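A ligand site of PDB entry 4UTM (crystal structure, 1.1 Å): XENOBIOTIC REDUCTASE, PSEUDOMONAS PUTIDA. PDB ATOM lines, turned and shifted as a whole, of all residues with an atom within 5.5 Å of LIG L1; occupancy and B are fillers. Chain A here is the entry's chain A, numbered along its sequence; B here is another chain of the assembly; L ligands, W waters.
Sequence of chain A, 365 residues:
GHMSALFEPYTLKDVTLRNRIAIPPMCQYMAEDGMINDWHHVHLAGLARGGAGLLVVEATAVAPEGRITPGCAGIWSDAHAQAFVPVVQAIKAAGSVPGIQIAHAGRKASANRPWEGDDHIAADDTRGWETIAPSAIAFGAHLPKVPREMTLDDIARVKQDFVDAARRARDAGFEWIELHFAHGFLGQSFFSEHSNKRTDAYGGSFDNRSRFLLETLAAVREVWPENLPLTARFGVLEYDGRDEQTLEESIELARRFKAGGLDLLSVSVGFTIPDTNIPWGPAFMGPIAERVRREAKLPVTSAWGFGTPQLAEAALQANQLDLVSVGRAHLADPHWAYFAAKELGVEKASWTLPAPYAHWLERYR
O9 of LIG L1 sits at hydrogen-bond distance from N of Gly 327 (2.7 Å).
The guanidinium group (NH1) of Arg 233 lies within hydrogen-bond range of an oxygen (O1) of LIG L1 (2.8 Å).
O7 of LIG L1 lies within hydrogen-bond range of N of Arg 328 (2.8 Å).
O7 of LIG L1 is in salt-bridge range of NE of Arg 328, 2.8 Å away.
The side-chain amide oxygen (OE1) of Gln 101 is in hydrogen-bond range of a nitrogen (N3) of LIG L1.
The backbone carbonyl oxygen (O) of Pro 25 lies within hydrogen-bond range of an oxygen (O3) of LIG L1 (2.9 Å).
An oxygen (O8) of LIG L1 lies within hydrogen-bond range of the backbone NH of Gly 305 (2.9 Å).
N of Cys 27 lies close to O2 of LIG L1.
The side-chain sulfur (SG) of Cys 27 lies within hydrogen-bond range of an oxygen (O2) of LIG L1 (3.2 Å).
The backbone NH of Ala 59 is in hydrogen-bond range of an oxygen (O2) of LIG L1.
N of Trp 304 sits at hydrogen-bond distance from O6 of LIG L1 (3.4 Å).
A ring nitrogen (NE2) of His 180 is in hydrogen-bond range of an oxygen (O1) of LIG L1 (3.3 Å).
A ring nitrogen (NE2) of His 180 lies within hydrogen-bond range of an oxygen (O2) of LG2 L2, at 2.9 Å.
An oxygen (O2) of LG2 L2 is in hydrogen-bond range of a ring nitrogen (ND1) of His 183 (2.8 Å).
N3 of LIG L1 lies close to O2 of LG2 L2 (3.3 Å).
The side-chain amide oxygen of Gln 101 sits close to the backbone NH of Ala 59 (3.4 Å).
The side-chain amide nitrogen (NE2) of Gln 101 sits at hydrogen-bond distance from the side-chain carboxylate (OE2) of Glu 178, 2.8 Å away.
The indole nitrogen (NE1) of Trp 360 of chain B lies close to the backbone carbonyl oxygen (O) of Pro 356 of chain B (3.5 Å).
The backbone carbonyl oxygen (O) of Met 26 lies within hydrogen-bond range of the side-chain amide nitrogen (NE2) of Gln 28 (3.1 Å).
N of Gln 28 lies within hydrogen-bond range of OE1 of Glu 58, at 3.0 Å.
Pro 24 touches LIG L1.
Met 26 touches LIG L1.
CA of Glu 58 touches O2 of LIG L1, at 3.9 Å.
His 183 touches LIG L1 (CE1 to O1, 3.4 Å).
Ala 303 touches LIG L1 (CB to O6, 3.6 Å).
Val 326 touches LIG L1.
Leu 331 touches LIG L1 (CD1 to C9, 3.99 Å).
Trp 360 of chain B touches LIG L1 (NE1 to C9, 3.1 Å).
Hydrophobic or aromatic side chains that line LIG L1: Pro 24, Pro 25, Met 26, Ala 59, His 180, His 183, Ala 303, Trp 304, Leu 331 and Trp 360 of chain B.
18 residues have an atom within 4 Å of LIG L1: Pro 24, Pro 25, Met 26, Cys 27, Glu 58, Ala 59, Gln 101, His 180, His 183, Arg 233, Ala 303, Trp 304, Gly 305, Val 326, Gly 327, Arg 328, Leu 331 and Trp 360 of chain B.
Along chain A the residues within 4 Å of LIG L1 span positions 24 to 331.
Water W2 lies within hydrogen-bond range of an oxygen (O9) of LIG L1 (2.7 Å), the backbone NH (N) of Ala 329 (2.8 Å) and the backbone NH (N) of Arg 328 (3.4 Å).
Water W1 bridges O8 of LIG L1 (2.8 Å) and NH2 of Arg 328 (3.4 Å).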
ATOM      1  N   PRO A  24      31.704  22.337 -11.152  1.00  0.00           N
ATOM      2  CA  PRO A  24      32.490  23.277 -11.946  1.00  0.00           C
ATOM      3  C   PRO A  24      31.744  24.599 -12.047  1.00  0.00           C
ATOM      4  O   PRO A  24      30.526  24.665 -11.814  1.00  0.00           O
ATOM      5  CB  PRO A  24      32.582  22.579 -13.314  1.00  0.00           C
ATOM      6  CG  PRO A  24      31.263  21.850 -13.401  1.00  0.00           C
ATOM      7  CD  PRO A  24      30.990  21.366 -12.002  1.00  0.00           C
ATOM      8  N   PRO A  25      32.457  25.653 -12.462  1.00  0.00           N
ATOM      9  CA  PRO A  25      31.809  26.952 -12.654  1.00  0.00           C
ATOM     10  C   PRO A  25      30.684  26.847 -13.675  1.00  0.00           C
ATOM     11  O   PRO A  25      30.853  26.300 -14.753  1.00  0.00           O
ATOM     12  CB  PRO A  25      32.954  27.842 -13.144  1.00  0.00           C
ATOM     13  CG  PRO A  25      33.988  26.882 -13.699  1.00  0.00           C
ATOM     14  CD  PRO A  25      33.896  25.688 -12.819  1.00  0.00           C
ATOM     15  N   MET A  26      29.524  27.404 -13.318  1.00  0.00           N
ATOM     16  CA  MET A  26      28.356  27.425 -14.198  1.00  0.00           C
ATOM     17  C   MET A  26      27.660  28.769 -14.103  1.00  0.00           C
ATOM     18  O   MET A  26      26.925  29.046 -13.149  1.00  0.00           O
ATOM     19  CB  MET A  26      27.355  26.300 -13.904  1.00  0.00           C
ATOM     20  CG  MET A  26      27.871  24.929 -14.308  1.00  0.00           C
ATOM     21  SD  MET A  26      26.663  23.615 -13.988  1.00  0.00           S
ATOM     22  CE  MET A  26      26.801  23.525 -12.218  1.00  0.00           C
ATOM     23  N   CYS A  27      27.900  29.609 -15.078  1.00  0.00           N
ATOM     24  CA  CYS A  27      27.216  30.881 -15.251  1.00  0.00           C
ATOM     25  C   CYS A  27      25.717  30.766 -15.058  1.00  0.00           C
ATOM     26  O   CYS A  27      25.074  29.864 -15.611  1.00  0.00           O
ATOM     27  CB  CYS A  27      27.485  31.467 -16.653  1.00  0.00           C
ATOM     28  SG  CYS A  27      29.117  32.211 -16.838  1.00  0.00           S
ATOM     29  N   GLN A  28      25.179  31.716 -14.293  1.00  0.00           N
ATOM     30  CA  GLN A  28      23.758  31.789 -14.002  1.00  0.00           C
ATOM     31  C   GLN A  28      23.040  32.924 -14.731  1.00  0.00           C
ATOM     32  O   GLN A  28      21.823  32.908 -14.837  1.00  0.00           O
ATOM     33  CB  GLN A  28      23.547  31.927 -12.491  1.00  0.00           C
ATOM     34  CG  GLN A  28      24.061  30.730 -11.717  1.00  0.00           C
ATOM     35  CD  GLN A  28      23.304  29.487 -12.025  1.00  0.00           C
ATOM     36  OE1 GLN A  28      22.145  29.337 -11.620  1.00  0.00           O
ATOM     37  NE2 GLN A  28      23.931  28.575 -12.775  1.00  0.00           N
ATOM     38  N   TYR A  29      23.794  33.925 -15.187  1.00  0.00           N
ATOM     39  CA  TYR A  29      23.243  35.023 -15.955  1.00  0.00           C
ATOM     40  C   TYR A  29      22.196  35.832 -15.181  1.00  0.00           C
ATOM     41  O   TYR A  29      21.292  36.411 -15.780  1.00  0.00           O
ATOM     42  CB  TYR A  29      22.710  34.563 -17.323  1.00  0.00           C
ATOM     43  CG  TYR A  29      23.670  33.667 -18.079  1.00  0.00           C
ATOM     44  CD1 TYR A  29      24.643  34.208 -18.911  1.00  0.00           C
ATOM     45  CD2 TYR A  29      23.637  32.295 -17.926  1.00  0.00           C
ATOM     46  CE1 TYR A  29      25.538  33.399 -19.599  1.00  0.00           C
ATOM     47  CE2 TYR A  29      24.534  31.482 -18.606  1.00  0.00           C
ATOM     48  CZ  TYR A  29      25.477  32.035 -19.433  1.00  0.00           C
ATOM     49  OH  TYR A  29      26.338  31.176 -20.101  1.00  0.00           O
ATOM     50  N   GLU A  58      30.771  30.364 -10.674  1.00  0.00           N
ATOM     51  CA  GLU A  58      30.760  30.721 -12.084  1.00  0.00           C
ATOM     52  C   GLU A  58      31.794  31.759 -12.482  1.00  0.00           C
ATOM     53  O   GLU A  58      32.216  32.586 -11.673  1.00  0.00           O
ATOM     54  CB  GLU A  58      29.389  31.304 -12.433  1.00  0.00           C
ATOM     55  CG  GLU A  58      29.022  32.603 -11.692  1.00  0.00           C
ATOM     56  CD  GLU A  58      27.517  32.867 -11.791  1.00  0.00           C
ATOM     57  OE1 GLU A  58      27.076  33.461 -12.816  1.00  0.00           O
ATOM     58  OE2 GLU A  58      26.792  32.469 -10.858  1.00  0.00           O
ATOM     59  N   ALA A  59      32.121  31.759 -13.780  1.00  0.00           N
ATOM     60  CA  ALA A  59      32.991  32.765 -14.366  1.00  0.00           C
ATOM     61  C   ALA A  59      32.590  34.155 -13.895  1.00  0.00           C
ATOM     62  O   ALA A  59      31.491  34.641 -14.185  1.00  0.00           O
ATOM     63  CB  ALA A  59      32.907  32.710 -15.877  1.00  0.00           C
ATOM     64  N   GLN A 101      35.969  30.996 -10.126  1.00  0.00           N
ATOM     65  CA  GLN A 101      36.633  31.147 -11.407  1.00  0.00           C
ATOM     66  C   GLN A 101      36.633  32.614 -11.793  1.00  0.00           C
ATOM     67  O   GLN A 101      35.551  33.197 -11.919  1.00  0.00           O
ATOM     68  CB  GLN A 101      35.910  30.308 -12.478  1.00  0.00           C
ATOM     69  CG  GLN A 101      36.649  30.322 -13.798  1.00  0.00           C
ATOM     70  CD  GLN A 101      35.850  29.683 -14.891  1.00  0.00           C
ATOM     71  OE1 GLN A 101      34.751  30.137 -15.186  1.00  0.00           O
ATOM     72  NE2 GLN A 101      36.368  28.614 -15.500  1.00  0.00           N
ATOM     73  N   GLU A 178      40.380  29.653  -9.642  1.00  0.00           N
ATOM     74  CA  GLU A 178      40.581  29.097 -10.984  1.00  0.00           C
ATOM     75  C   GLU A 178      40.671  30.233 -11.976  1.00  0.00           C
ATOM     76  O   GLU A 178      39.724  31.011 -12.124  1.00  0.00           O
ATOM     77  CB  GLU A 178      39.443  28.133 -11.349  1.00  0.00           C
ATOM     78  CG  GLU A 178      39.655  27.456 -12.699  1.00  0.00           C
ATOM     79  CD  GLU A 178      38.515  26.501 -13.035  1.00  0.00           C
ATOM     80  OE1 GLU A 178      38.374  25.461 -12.364  1.00  0.00           O
ATOM     81  OE2 GLU A 178      37.746  26.773 -13.960  1.00  0.00           O
ATOM     82  N   HIS A 180      40.392  31.507 -15.640  1.00  0.00           N
ATOM     83  CA  HIS A 180      39.661  31.018 -16.806  1.00  0.00           C
ATOM     84  C   HIS A 180      40.423  31.296 -18.098  1.00  0.00           C
ATOM     85  O   HIS A 180      40.247  32.320 -18.745  1.00  0.00           O
ATOM     86  CB  HIS A 180      38.289  31.670 -16.883  1.00  0.00           C
ATOM     87  CG  HIS A 180      37.373  30.932 -17.790  1.00  0.00           C
ATOM     88  ND1 HIS A 180      37.789  29.918 -18.619  1.00  0.00           N
ATOM     89  CD2 HIS A 180      36.021  31.012 -17.918  1.00  0.00           C
ATOM     90  CE1 HIS A 180      36.733  29.406 -19.219  1.00  0.00           C
ATOM     91  NE2 HIS A 180      35.649  30.053 -18.814  1.00  0.00           N
ATOM     92  N   HIS A 183      37.899  28.040 -23.300  1.00  0.00           N
ATOM     93  CA  HIS A 183      36.579  28.314 -23.878  1.00  0.00           C
ATOM     94  C   HIS A 183      36.544  29.519 -24.793  1.00  0.00           C
ATOM     95  O   HIS A 183      35.499  30.099 -25.039  1.00  0.00           O
ATOM     96  CB  HIS A 183      35.480  28.331 -22.802  1.00  0.00           C
ATOM     97  CG  HIS A 183      35.399  27.041 -22.024  1.00  0.00           C
ATOM     98  ND1 HIS A 183      34.650  26.912 -20.881  1.00  0.00           N
ATOM     99  CD2 HIS A 183      35.975  25.821 -22.226  1.00  0.00           C
ATOM    100  CE1 HIS A 183      34.776  25.679 -20.411  1.00  0.00           C
ATOM    101  NE2 HIS A 183      35.556  24.990 -21.222  1.00  0.00           N
ATOM    102  N   ARG A 233      41.659  26.744 -15.726  1.00  0.00           N
ATOM    103  CA  ARG A 233      40.961  25.976 -16.744  1.00  0.00           C
ATOM    104  C   ARG A 233      41.593  26.346 -18.075  1.00  0.00           C
ATOM    105  O   ARG A 233      41.817  27.527 -18.368  1.00  0.00           O
ATOM    106  CB  ARG A 233      39.463  26.240 -16.751  1.00  0.00           C
ATOM    107  CG  ARG A 233      38.660  25.149 -17.494  1.00  0.00           C
ATOM    108  CD  ARG A 233      37.173  25.199 -17.252  1.00  0.00           C
ATOM    109  NE  ARG A 233      36.610  23.851 -17.350  1.00  0.00           N
ATOM    110  CZ  ARG A 233      35.323  23.566 -17.164  1.00  0.00           C
ATOM    111  NH1 ARG A 233      34.419  24.520 -16.997  1.00  0.00           N
ATOM    112  NH2 ARG A 233      34.979  22.270 -17.129  1.00  0.00           N
ATOM    113  N   ALA A 303      35.329  17.595 -17.222  1.00  0.00           N
ATOM    114  CA  ALA A 303      33.880  17.510 -17.171  1.00  0.00           C
ATOM    115  C   ALA A 303      33.429  17.124 -18.574  1.00  0.00           C
ATOM    116  O   ALA A 303      34.231  16.645 -19.363  1.00  0.00           O
ATOM    117  CB  ALA A 303      33.287  18.847 -16.748  1.00  0.00           C
ATOM    118  N   TRP A 304      32.075  16.889 -18.563  1.00  0.00           N
ATOM    119  CA  TRP A 304      31.194  16.593 -19.694  1.00  0.00           C
ATOM    120  C   TRP A 304      30.742  15.147 -19.645  1.00  0.00           C
ATOM    121  O   TRP A 304      31.448  14.250 -20.106  1.00  0.00           O
ATOM    122  CB  TRP A 304      31.744  16.926 -21.088  1.00  0.00           C
ATOM    123  CG  TRP A 304      30.641  16.740 -22.112  1.00  0.00           C
ATOM    124  CD1 TRP A 304      30.174  15.551 -22.628  1.00  0.00           C
ATOM    125  CD2 TRP A 304      29.836  17.768 -22.693  1.00  0.00           C
ATOM    126  NE1 TRP A 304      29.147  15.791 -23.509  1.00  0.00           N
ATOM    127  CE2 TRP A 304      28.919  17.146 -23.561  1.00  0.00           C
ATOM    128  CE3 TRP A 304      29.799  19.157 -22.566  1.00  0.00           C
ATOM    129  CZ2 TRP A 304      27.978  17.864 -24.298  1.00  0.00           C
ATOM    130  CZ3 TRP A 304      28.870  19.871 -23.297  1.00  0.00           C
ATOM    131  CH2 TRP A 304      27.975  19.223 -24.163  1.00  0.00           C
ATOM    132  N   GLY A 305      29.564  14.976 -19.103  1.00  0.00           N
ATOM    133  CA  GLY A 305      28.978  13.680 -19.071  1.00  0.00           C
ATOM    134  C   GLY A 305      29.435  12.781 -17.954  1.00  0.00           C
ATOM    135  O   GLY A 305      29.175  11.569 -18.043  1.00  0.00           O
ATOM    136  N   PHE A 306      30.093  13.297 -16.916  1.00  0.00           N
ATOM    137  CA  PHE A 306      30.459  12.507 -15.746  1.00  0.00           C
ATOM    138  C   PHE A 306      29.376  12.346 -14.699  1.00  0.00           C
ATOM    139  O   PHE A 306      29.653  11.745 -13.730  1.00  0.00           O
ATOM    140  CB  PHE A 306      31.791  12.989 -15.135  1.00  0.00           C
ATOM    141  CG  PHE A 306      33.018  12.811 -15.985  1.00  0.00           C
ATOM    142  CD1 PHE A 306      33.772  11.651 -16.012  1.00  0.00           C
ATOM    143  CD2 PHE A 306      33.505  13.855 -16.755  1.00  0.00           C
ATOM    144  CE1 PHE A 306      34.929  11.613 -16.741  1.00  0.00           C
ATOM    145  CE2 PHE A 306      34.635  13.763 -17.504  1.00  0.00           C
ATOM    146  CZ  PHE A 306      35.352  12.634 -17.515  1.00  0.00           C
ATOM    147  N   GLY A 307      28.151  12.886 -14.884  1.00  0.00           N
ATOM    148  CA  GLY A 307      27.032  12.757 -13.985  1.00  0.00           C
ATOM    149  C   GLY A 307      26.343  11.395 -13.884  1.00  0.00           C
ATOM    150  O   GLY A 307      25.380  11.191 -13.194  1.00  0.00           O
ATOM    151  N   SER A 325      34.399  16.677 -12.206  1.00  0.00           N
ATOM    152  CA  SER A 325      33.497  17.813 -12.250  1.00  0.00           C
ATOM    153  C   SER A 325      32.166  17.394 -12.852  1.00  0.00           C
ATOM    154  O   SER A 325      32.120  16.838 -13.946  1.00  0.00           O
ATOM    155  CB  SER A 325      34.126  18.954 -13.027  1.00  0.00           C
ATOM    156  OG  SER A 325      35.291  19.436 -12.349  1.00  0.00           O
ATOM    157  N   VAL A 326      31.085  17.715 -12.126  1.00  0.00           N
ATOM    158  CA  VAL A 326      29.723  17.328 -12.489  1.00  0.00           C
ATOM    159  C   VAL A 326      28.853  18.584 -12.490  1.00  0.00           C
ATOM    160  O   VAL A 326      28.572  19.156 -11.433  1.00  0.00           O
ATOM    161  CB  VAL A 326      29.185  16.258 -11.515  1.00  0.00           C
ATOM    162  CG1 VAL A 326      27.737  15.913 -11.850  1.00  0.00           C
ATOM    163  CG2 VAL A 326      30.087  15.025 -11.547  1.00  0.00           C
ATOM    164  N   GLY A 327      28.470  19.025 -13.675  1.00  0.00           N
ATOM    165  CA  GLY A 327      27.784  20.301 -13.856  1.00  0.00           C
ATOM    166  C   GLY A 327      26.277  20.189 -13.989  1.00  0.00           C
ATOM    167  O   GLY A 327      25.534  20.399 -13.032  1.00  0.00           O
ATOM    168  N   ARG A 328      25.797  19.849 -15.180  1.00  0.00           N
ATOM    169  CA  ARG A 328      24.353  19.848 -15.440  1.00  0.00           C
ATOM    170  C   ARG A 328      23.578  18.930 -14.508  1.00  0.00           C
ATOM    171  O   ARG A 328      22.447  19.255 -14.142  1.00  0.00           O
ATOM    172  CB  ARG A 328      24.048  19.551 -16.902  1.00  0.00           C
ATOM    173  CG  ARG A 328      24.330  20.753 -17.780  1.00  0.00           C
ATOM    174  CD  ARG A 328      24.350  20.450 -19.246  1.00  0.00           C
ATOM    175  NE  ARG A 328      25.521  19.642 -19.552  1.00  0.00           N
ATOM    176  CZ  ARG A 328      25.786  19.143 -20.754  1.00  0.00           C
ATOM    177  NH1 ARG A 328      24.960  19.397 -21.763  1.00  0.00           N
ATOM    178  NH2 ARG A 328      26.855  18.395 -20.948  1.00  0.00           N
ATOM    179  N   ALA A 329      24.148  17.801 -14.117  1.00  0.00           N
ATOM    180  CA  ALA A 329      23.419  16.920 -13.204  1.00  0.00           C
ATOM    181  C   ALA A 329      23.093  17.613 -11.879  1.00  0.00           C
ATOM    182  O   ALA A 329      22.087  17.270 -11.237  1.00  0.00           O
ATOM    183  CB  ALA A 329      24.181  15.654 -12.948  1.00  0.00           C
ATOM    184  N   LEU A 331      22.426  20.952 -11.698  1.00  0.00           N
ATOM    185  CA  LEU A 331      21.295  21.826 -11.995  1.00  0.00           C
ATOM    186  C   LEU A 331      19.995  21.028 -11.924  1.00  0.00           C
ATOM    187  O   LEU A 331      18.980  21.501 -11.411  1.00  0.00           O
ATOM    188  CB  LEU A 331      21.443  22.472 -13.374  1.00  0.00           C
ATOM    189  CG  LEU A 331      22.752  23.232 -13.621  1.00  0.00           C
ATOM    190  CD1 LEU A 331      22.733  23.866 -14.999  1.00  0.00           C
ATOM    191  CD2 LEU A 331      23.046  24.263 -12.531  1.00  0.00           C
ATOM    192  N   PRO B 356      17.775  29.704 -15.633  1.00  0.00           N
ATOM    193  CA  PRO B 356      19.204  29.362 -15.516  1.00  0.00           C
ATOM    194  C   PRO B 356      19.468  27.863 -15.363  1.00  0.00           C
ATOM    195  O   PRO B 356      20.623  27.455 -15.522  1.00  0.00           O
ATOM    196  CB  PRO B 356      19.663  30.126 -14.292  1.00  0.00           C
ATOM    197  CG  PRO B 356      18.683  31.249 -14.151  1.00  0.00           C
ATOM    198  CD  PRO B 356      17.358  30.653 -14.578  1.00  0.00           C
ATOM    199  N   TRP B 360      19.372  24.616 -20.010  1.00  0.00           N
ATOM    200  CA  TRP B 360      20.439  23.639 -20.195  1.00  0.00           C
ATOM    201  C   TRP B 360      19.980  22.205 -20.101  1.00  0.00           C
ATOM    202  O   TRP B 360      20.704  21.286 -20.474  1.00  0.00           O
ATOM    203  CB  TRP B 360      21.543  23.887 -19.162  1.00  0.00           C
ATOM    204  CG  TRP B 360      21.958  25.292 -19.163  1.00  0.00           C
ATOM    205  CD1 TRP B 360      21.609  26.239 -18.261  1.00  0.00           C
ATOM    206  CD2 TRP B 360      22.715  25.937 -20.175  1.00  0.00           C
ATOM    207  NE1 TRP B 360      22.119  27.449 -18.644  1.00  0.00           N
ATOM    208  CE2 TRP B 360      22.813  27.286 -19.819  1.00  0.00           C
ATOM    209  CE3 TRP B 360      23.318  25.499 -21.360  1.00  0.00           C
ATOM    210  CZ2 TRP B 360      23.510  28.191 -20.566  1.00  0.00           C
ATOM    211  CZ3 TRP B 360      23.992  26.400 -22.115  1.00  0.00           C
ATOM    212  CH2 TRP B 360      24.085  27.748 -21.710  1.00  0.00           C
HETATM  213  C1  LIG L   1      28.891  26.052 -18.053  1.00  0.00           C
HETATM  214  N1  LIG L   1      30.282  25.829 -18.214  1.00  0.00           N
HETATM  215  C2  LIG L   1      31.177  26.845 -17.753  1.00  0.00           C
HETATM  216  N2  LIG L   1      32.485  26.556 -17.851  1.00  0.00           N
HETATM  217  C3  LIG L   1      33.384  27.495 -17.349  1.00  0.00           C
HETATM  218  O1  LIG L   1      34.594  27.258 -17.388  1.00  0.00           O
HETATM  219  N3  LIG L   1      32.848  28.643 -16.692  1.00  0.00           N
HETATM  220  C4  LIG L   1      31.533  28.927 -16.583  1.00  0.00           C
HETATM  221  O2  LIG L   1      31.152  29.899 -15.882  1.00  0.00           O
HETATM  222  C5  LIG L   1      30.681  28.054 -17.300  1.00  0.00           C
HETATM  223  N4  LIG L   1      29.316  28.366 -17.348  1.00  0.00           N
HETATM  224  C6  LIG L   1      28.431  27.281 -17.648  1.00  0.00           C
HETATM  225  C7  LIG L   1      27.059  27.495 -17.428  1.00  0.00           C
HETATM  226  C8  LIG L   1      26.153  26.417 -17.529  1.00  0.00           C
HETATM  227  C9  LIG L   1      24.724  26.592 -17.122  1.00  0.00           C
HETATM  228  C10 LIG L   1      26.640  25.158 -18.017  1.00  0.00           C
HETATM  229  C11 LIG L   1      25.715  24.013 -18.183  1.00  0.00           C
HETATM  230  C12 LIG L   1      27.979  24.994 -18.306  1.00  0.00           C
HETATM  231  C13 LIG L   1      30.823  24.466 -18.503  1.00  0.00           C
HETATM  232  C14 LIG L   1      30.669  23.536 -17.298  1.00  0.00           C
HETATM  233  O3  LIG L   1      31.599  23.977 -16.270  1.00  0.00           O
HETATM  234  C15 LIG L   1      30.944  22.051 -17.612  1.00  0.00           C
HETATM  235  O4  LIG L   1      32.286  21.975 -18.151  1.00  0.00           O
HETATM  236  C16 LIG L   1      29.977  21.493 -18.667  1.00  0.00           C
HETATM  237  O5  LIG L   1      28.614  21.813 -18.275  1.00  0.00           O
HETATM  238  C17 LIG L   1      30.148  19.978 -18.846  1.00  0.00           C
HETATM  239  O6  LIG L   1      29.868  19.273 -17.656  1.00  0.00           O
HETATM  240  P1  LIG L   1      28.480  18.489 -17.431  1.00  0.00           P
HETATM  241  O7  LIG L   1      27.384  19.539 -17.433  1.00  0.00           O
HETATM  242  O8  LIG L   1      28.297  17.529 -18.626  1.00  0.00           O
HETATM  243  O9  LIG L   1      28.632  17.783 -16.100  1.00  0.00           O
HETATM  244  C1  LG2 L   2      27.939  28.126 -21.023  1.00  0.00           C
HETATM  245  C2  LG2 L   2      27.682  26.893 -21.573  1.00  0.00           C
HETATM  246  C3  LG2 L   2      28.676  26.010 -21.885  1.00  0.00           C
HETATM  247  C4  LG2 L   2      29.960  26.342 -21.574  1.00  0.00           C
HETATM  248  C5  LG2 L   2      30.219  27.615 -21.015  1.00  0.00           C
HETATM  249  C6  LG2 L   2      29.249  28.540 -20.724  1.00  0.00           C
HETATM  250  C7  LG2 L   2      29.621  29.775 -20.140  1.00  0.00           C
HETATM  251  C8  LG2 L   2      30.978  30.029 -19.871  1.00  0.00           C
HETATM  252  C9  LG2 L   2      31.961  29.056 -20.157  1.00  0.00           C
HETATM  253  O1  LG2 L   2      31.515  27.922 -20.768  1.00  0.00           O
HETATM  254  O2  LG2 L   2      33.105  29.087 -19.948  1.00  0.00           O
HETATM  255  O3  LG2 L   2      31.058  25.518 -21.782  1.00  0.00           O
HETATM  256  O   HOH W   1      26.050  15.904 -18.769  1.00  0.00           O
HETATM  257  O   HOH W   2      26.405  16.476 -15.183  1.00  0.00           O
HETATM  258  O   HOH W   3      30.743  16.098 -16.190  1.00  0.00           O
